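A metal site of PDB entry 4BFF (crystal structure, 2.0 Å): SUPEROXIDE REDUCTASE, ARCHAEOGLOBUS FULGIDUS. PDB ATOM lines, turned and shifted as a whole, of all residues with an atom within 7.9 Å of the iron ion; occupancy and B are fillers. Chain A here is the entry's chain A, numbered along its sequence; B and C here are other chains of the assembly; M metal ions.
Five residues have an atom within 4 Å of the iron ion: His 14, His 40, His 46, Cys 110 and His 113.
The iron ion is bound by NE2 of His 14, NE2 of His 46, NE2 of His 40, ND1 of His 113 and SG of Cys 110.
N of His 14 is in hydrogen-bond range of OE2 of Glu 12, at 3.0 Å. O of His 113 is in hydrogen-bond range of NE1 of Trp 116, 3.0 Å away. The side-chain sulfur (SG) of Cys 110 lies close to the backbone NH (N) of Ile 112.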
ATOM      1  N   GLU A  12     -10.313  23.567  -0.025  1.00  0.00           N
ATOM      2  CA  GLU A  12     -10.802  24.337  -1.166  1.00  0.00           C
ATOM      3  C   GLU A  12     -11.924  23.618  -1.904  1.00  0.00           C
ATOM      4  O   GLU A  12     -11.726  22.566  -2.525  1.00  0.00           O
ATOM      5  CB  GLU A  12      -9.654  24.741  -2.098  1.00  0.00           C
ATOM      6  CG  GLU A  12     -10.041  25.417  -3.429  1.00  0.00           C
ATOM      7  CD  GLU A  12     -10.907  26.653  -3.266  1.00  0.00           C
ATOM      8  OE1 GLU A  12     -10.378  27.718  -2.884  1.00  0.00           O
ATOM      9  OE2 GLU A  12     -12.124  26.562  -3.545  1.00  0.00           O
ATOM     10  N   LYS A  13     -13.117  24.203  -1.807  1.00  0.00           N
ATOM     11  CA  LYS A  13     -14.343  23.641  -2.358  1.00  0.00           C
ATOM     12  C   LYS A  13     -14.279  23.369  -3.872  1.00  0.00           C
ATOM     13  O   LYS A  13     -14.999  22.519  -4.385  1.00  0.00           O
ATOM     14  CB  LYS A  13     -15.514  24.599  -2.074  1.00  0.00           C
ATOM     15  CG  LYS A  13     -15.398  25.955  -2.794  1.00  0.00           C
ATOM     16  CD  LYS A  13     -16.631  26.853  -2.613  1.00  0.00           C
ATOM     17  CE  LYS A  13     -16.633  27.501  -1.236  1.00  0.00           C
ATOM     18  NZ  LYS A  13     -17.829  28.380  -1.020  1.00  0.00           N
ATOM     19  N   HIS A  14     -13.450  24.100  -4.599  1.00  0.00           N
ATOM     20  CA  HIS A  14     -13.439  24.016  -6.064  1.00  0.00           C
ATOM     21  C   HIS A  14     -12.624  22.827  -6.607  1.00  0.00           C
ATOM     22  O   HIS A  14     -12.846  22.415  -7.750  1.00  0.00           O
ATOM     23  CB  HIS A  14     -12.939  25.327  -6.697  1.00  0.00           C
ATOM     24  CG  HIS A  14     -13.954  26.439  -6.707  1.00  0.00           C
ATOM     25  ND1 HIS A  14     -13.874  27.533  -5.880  1.00  0.00           N
ATOM     26  CD2 HIS A  14     -15.078  26.627  -7.455  1.00  0.00           C
ATOM     27  CE1 HIS A  14     -14.888  28.347  -6.111  1.00  0.00           C
ATOM     28  NE2 HIS A  14     -15.632  27.828  -7.060  1.00  0.00           N
ATOM     29  N   VAL A  34     -16.467  17.514  -7.270  1.00  0.00           N
ATOM     30  CA  VAL A  34     -16.087  18.821  -6.775  1.00  0.00           C
ATOM     31  C   VAL A  34     -16.964  19.149  -5.570  1.00  0.00           C
ATOM     32  O   VAL A  34     -18.184  19.009  -5.625  1.00  0.00           O
ATOM     33  CB  VAL A  34     -16.273  19.913  -7.866  1.00  0.00           C
ATOM     34  CG1 VAL A  34     -15.967  21.274  -7.308  1.00  0.00           C
ATOM     35  CG2 VAL A  34     -15.401  19.612  -9.103  1.00  0.00           C
ATOM     36  N   HIS A  40     -19.760  22.988  -2.754  1.00  0.00           N
ATOM     37  CA  HIS A  40     -19.832  24.148  -3.631  1.00  0.00           C
ATOM     38  C   HIS A  40     -21.301  24.360  -3.998  1.00  0.00           C
ATOM     39  O   HIS A  40     -22.058  23.385  -4.126  1.00  0.00           O
ATOM     40  CB  HIS A  40     -18.985  23.890  -4.872  1.00  0.00           C
ATOM     41  CG  HIS A  40     -18.940  25.046  -5.818  1.00  0.00           C
ATOM     42  ND1 HIS A  40     -19.908  25.270  -6.767  1.00  0.00           N
ATOM     43  CD2 HIS A  40     -18.035  26.047  -5.952  1.00  0.00           C
ATOM     44  CE1 HIS A  40     -19.609  26.358  -7.456  1.00  0.00           C
ATOM     45  NE2 HIS A  40     -18.480  26.856  -6.979  1.00  0.00           N
ATOM     46  N   PRO A  41     -21.708  25.628  -4.157  1.00  0.00           N
ATOM     47  CA  PRO A  41     -23.066  26.040  -4.546  1.00  0.00           C
ATOM     48  C   PRO A  41     -23.535  25.404  -5.842  1.00  0.00           C
ATOM     49  O   PRO A  41     -22.707  24.991  -6.651  1.00  0.00           O
ATOM     50  CB  PRO A  41     -22.904  27.567  -4.733  1.00  0.00           C
ATOM     51  CG  PRO A  41     -21.832  27.935  -3.827  1.00  0.00           C
ATOM     52  CD  PRO A  41     -20.867  26.780  -3.789  1.00  0.00           C
ATOM     53  N   HIS A  46     -24.427  30.428 -10.100  1.00  0.00           N
ATOM     54  CA  HIS A  46     -23.108  29.938  -9.718  1.00  0.00           C
ATOM     55  C   HIS A  46     -23.101  28.407  -9.622  1.00  0.00           C
ATOM     56  O   HIS A  46     -23.900  27.826  -8.893  1.00  0.00           O
ATOM     57  CB  HIS A  46     -22.717  30.593  -8.387  1.00  0.00           C
ATOM     58  CG  HIS A  46     -21.346  30.255  -7.905  1.00  0.00           C
ATOM     59  ND1 HIS A  46     -20.912  30.508  -6.614  1.00  0.00           N
ATOM     60  CD2 HIS A  46     -20.286  29.677  -8.535  1.00  0.00           C
ATOM     61  CE1 HIS A  46     -19.679  30.103  -6.468  1.00  0.00           C
ATOM     62  NE2 HIS A  46     -19.260  29.599  -7.627  1.00  0.00           N
ATOM     63  N   HIS A  47     -22.208  27.747 -10.372  1.00  0.00           N
ATOM     64  CA  HIS A  47     -22.227  26.269 -10.456  1.00  0.00           C
ATOM     65  C   HIS A  47     -21.010  25.674 -11.151  1.00  0.00           C
ATOM     66  O   HIS A  47     -20.320  26.369 -11.923  1.00  0.00           O
ATOM     67  CB  HIS A  47     -23.474  25.794 -11.213  1.00  0.00           C
ATOM     68  CG  HIS A  47     -23.639  26.440 -12.560  1.00  0.00           C
ATOM     69  ND1 HIS A  47     -24.599  27.399 -12.823  1.00  0.00           N
ATOM     70  CD2 HIS A  47     -22.916  26.314 -13.704  1.00  0.00           C
ATOM     71  CE1 HIS A  47     -24.487  27.801 -14.072  1.00  0.00           C
ATOM     72  NE2 HIS A  47     -23.475  27.163 -14.633  1.00  0.00           N
ATOM     73  N   ILE A  48     -20.766  24.393 -10.868  1.00  0.00           N
ATOM     74  CA  ILE A  48     -19.789  23.550 -11.586  1.00  0.00           C
ATOM     75  C   ILE A  48     -20.371  22.980 -12.879  1.00  0.00           C
ATOM     76  O   ILE A  48     -21.234  22.088 -12.864  1.00  0.00           O
ATOM     77  CB  ILE A  48     -19.322  22.333 -10.730  1.00  0.00           C
ATOM     78  CG1 ILE A  48     -18.701  22.813  -9.400  1.00  0.00           C
ATOM     79  CG2 ILE A  48     -18.386  21.385 -11.537  1.00  0.00           C
ATOM     80  CD1 ILE A  48     -17.847  24.055  -9.498  1.00  0.00           C
ATOM     81  N   TYR A 109     -14.485  23.120 -14.018  1.00  0.00           N
ATOM     82  CA  TYR A 109     -14.783  24.518 -14.318  1.00  0.00           C
ATOM     83  C   TYR A 109     -16.000  25.019 -13.548  1.00  0.00           C
ATOM     84  O   TYR A 109     -17.075  24.430 -13.639  1.00  0.00           O
ATOM     85  CB  TYR A 109     -15.026  24.708 -15.823  1.00  0.00           C
ATOM     86  CG  TYR A 109     -15.388  26.131 -16.248  1.00  0.00           C
ATOM     87  CD1 TYR A 109     -14.461  27.165 -16.168  1.00  0.00           C
ATOM     88  CD2 TYR A 109     -16.646  26.426 -16.753  1.00  0.00           C
ATOM     89  CE1 TYR A 109     -14.781  28.480 -16.569  1.00  0.00           C
ATOM     90  CE2 TYR A 109     -16.980  27.731 -17.150  1.00  0.00           C
ATOM     91  CZ  TYR A 109     -16.039  28.752 -17.055  1.00  0.00           C
ATOM     92  OH  TYR A 109     -16.361  30.047 -17.459  1.00  0.00           O
ATOM     93  N   CYS A 110     -15.804  26.088 -12.795  1.00  0.00           N
ATOM     94  CA  CYS A 110     -16.894  26.845 -12.195  1.00  0.00           C
ATOM     95  C   CYS A 110     -17.199  28.033 -13.105  1.00  0.00           C
ATOM     96  O   CYS A 110     -16.275  28.718 -13.531  1.00  0.00           O
ATOM     97  CB  CYS A 110     -16.480  27.348 -10.810  1.00  0.00           C
ATOM     98  SG  CYS A 110     -17.701  28.457 -10.030  1.00  0.00           S
ATOM     99  N   ASN A 111     -18.466  28.273 -13.401  1.00  0.00           N
ATOM    100  CA  ASN A 111     -18.871  29.389 -14.277  1.00  0.00           C
ATOM    101  C   ASN A 111     -18.445  30.795 -13.835  1.00  0.00           C
ATOM    102  O   ASN A 111     -18.565  31.737 -14.610  1.00  0.00           O
ATOM    103  CB  ASN A 111     -20.385  29.375 -14.555  1.00  0.00           C
ATOM    104  CG  ASN A 111     -21.198  29.875 -13.373  1.00  0.00           C
ATOM    105  OD1 ASN A 111     -20.776  29.727 -12.224  1.00  0.00           O
ATOM    106  ND2 ASN A 111     -22.362  30.471 -13.648  1.00  0.00           N
ATOM    107  N   ILE A 112     -17.983  30.933 -12.593  1.00  0.00           N
ATOM    108  CA  ILE A 112     -17.506  32.239 -12.121  1.00  0.00           C
ATOM    109  C   ILE A 112     -16.099  32.221 -11.498  1.00  0.00           C
ATOM    110  O   ILE A 112     -15.456  33.265 -11.389  1.00  0.00           O
ATOM    111  CB  ILE A 112     -18.496  32.925 -11.134  1.00  0.00           C
ATOM    112  CG1 ILE A 112     -18.486  32.194  -9.781  1.00  0.00           C
ATOM    113  CG2 ILE A 112     -19.903  33.011 -11.736  1.00  0.00           C
ATOM    114  CD1 ILE A 112     -19.303  32.891  -8.737  1.00  0.00           C
ATOM    115  N   HIS A 113     -15.625  31.042 -11.109  1.00  0.00           N
ATOM    116  CA  HIS A 113     -14.374  30.899 -10.364  1.00  0.00           C
ATOM    117  C   HIS A 113     -13.294  30.166 -11.163  1.00  0.00           C
ATOM    118  O   HIS A 113     -12.338  29.641 -10.583  1.00  0.00           O
ATOM    119  CB  HIS A 113     -14.602  30.181  -9.014  1.00  0.00           C
ATOM    120  CG  HIS A 113     -15.277  31.034  -7.973  1.00  0.00           C
ATOM    121  ND1 HIS A 113     -16.436  30.661  -7.340  1.00  0.00           N
ATOM    122  CD2 HIS A 113     -14.931  32.237  -7.453  1.00  0.00           C
ATOM    123  CE1 HIS A 113     -16.787  31.588  -6.475  1.00  0.00           C
ATOM    124  NE2 HIS A 113     -15.882  32.553  -6.515  1.00  0.00           N
ATOM    125  N   GLY A 114     -13.461  30.117 -12.481  1.00  0.00           N
ATOM    126  CA  GLY A 114     -12.430  29.617 -13.378  1.00  0.00           C
ATOM    127  C   GLY A 114     -12.215  28.097 -13.408  1.00  0.00           C
ATOM    128  O   GLY A 114     -13.092  27.315 -13.019  1.00  0.00           O
ATOM    129  N   TRP A 116      -9.984  24.464 -12.756  1.00  0.00           N
ATOM    130  CA  TRP A 116      -9.329  23.763 -11.651  1.00  0.00           C
ATOM    131  C   TRP A 116      -8.780  22.419 -12.103  1.00  0.00           C
ATOM    132  O   TRP A 116      -9.303  21.804 -13.035  1.00  0.00           O
ATOM    133  CB  TRP A 116     -10.322  23.558 -10.511  1.00  0.00           C
ATOM    134  CG  TRP A 116     -10.708  24.862  -9.937  1.00  0.00           C
ATOM    135  CD1 TRP A 116     -11.658  25.724 -10.408  1.00  0.00           C
ATOM    136  CD2 TRP A 116     -10.110  25.511  -8.813  1.00  0.00           C
ATOM    137  NE1 TRP A 116     -11.687  26.855  -9.646  1.00  0.00           N
ATOM    138  CE2 TRP A 116     -10.752  26.748  -8.661  1.00  0.00           C
ATOM    139  CE3 TRP A 116      -9.092  25.161  -7.915  1.00  0.00           C
ATOM    140  CZ2 TRP A 116     -10.422  27.641  -7.631  1.00  0.00           C
ATOM    141  CZ3 TRP A 116      -8.754  26.047  -6.905  1.00  0.00           C
ATOM    142  CH2 TRP A 116      -9.425  27.268  -6.768  1.00  0.00           C
ATOM    143  N   VAL B  78     -18.302  36.664 -10.306  1.00  0.00           N
ATOM    144  CA  VAL B  78     -18.200  36.806  -8.859  1.00  0.00           C
ATOM    145  C   VAL B  78     -18.983  38.013  -8.310  1.00  0.00           C
ATOM    146  O   VAL B  78     -19.289  38.067  -7.113  1.00  0.00           O
ATOM    147  CB  VAL B  78     -16.721  36.960  -8.433  1.00  0.00           C
ATOM    148  CG1 VAL B  78     -15.992  35.646  -8.580  1.00  0.00           C
ATOM    149  CG2 VAL B  78     -16.039  38.073  -9.268  1.00  0.00           C
ATOM    150  N   PHE C  62     -10.865  36.011 -12.750  1.00  0.00           N
ATOM    151  CA  PHE C  62     -11.038  34.658 -13.282  1.00  0.00           C
ATOM    152  C   PHE C  62     -11.266  34.628 -14.812  1.00  0.00           C
ATOM    153  O   PHE C  62     -11.850  35.558 -15.376  1.00  0.00           O
ATOM    154  CB  PHE C  62     -12.180  33.930 -12.539  1.00  0.00           C
ATOM    155  CG  PHE C  62     -11.897  33.687 -11.091  1.00  0.00           C
ATOM    156  CD1 PHE C  62     -11.048  32.669 -10.687  1.00  0.00           C
ATOM    157  CD2 PHE C  62     -12.457  34.483 -10.107  1.00  0.00           C
ATOM    158  CE1 PHE C  62     -10.780  32.446  -9.353  1.00  0.00           C
ATOM    159  CE2 PHE C  62     -12.193  34.268  -8.762  1.00  0.00           C
ATOM    160  CZ  PHE C  62     -11.363  33.246  -8.390  1.00  0.00           C
HETATM  161 FE    FE M   1     -17.396  28.673  -7.653  1.00  0.00          FE
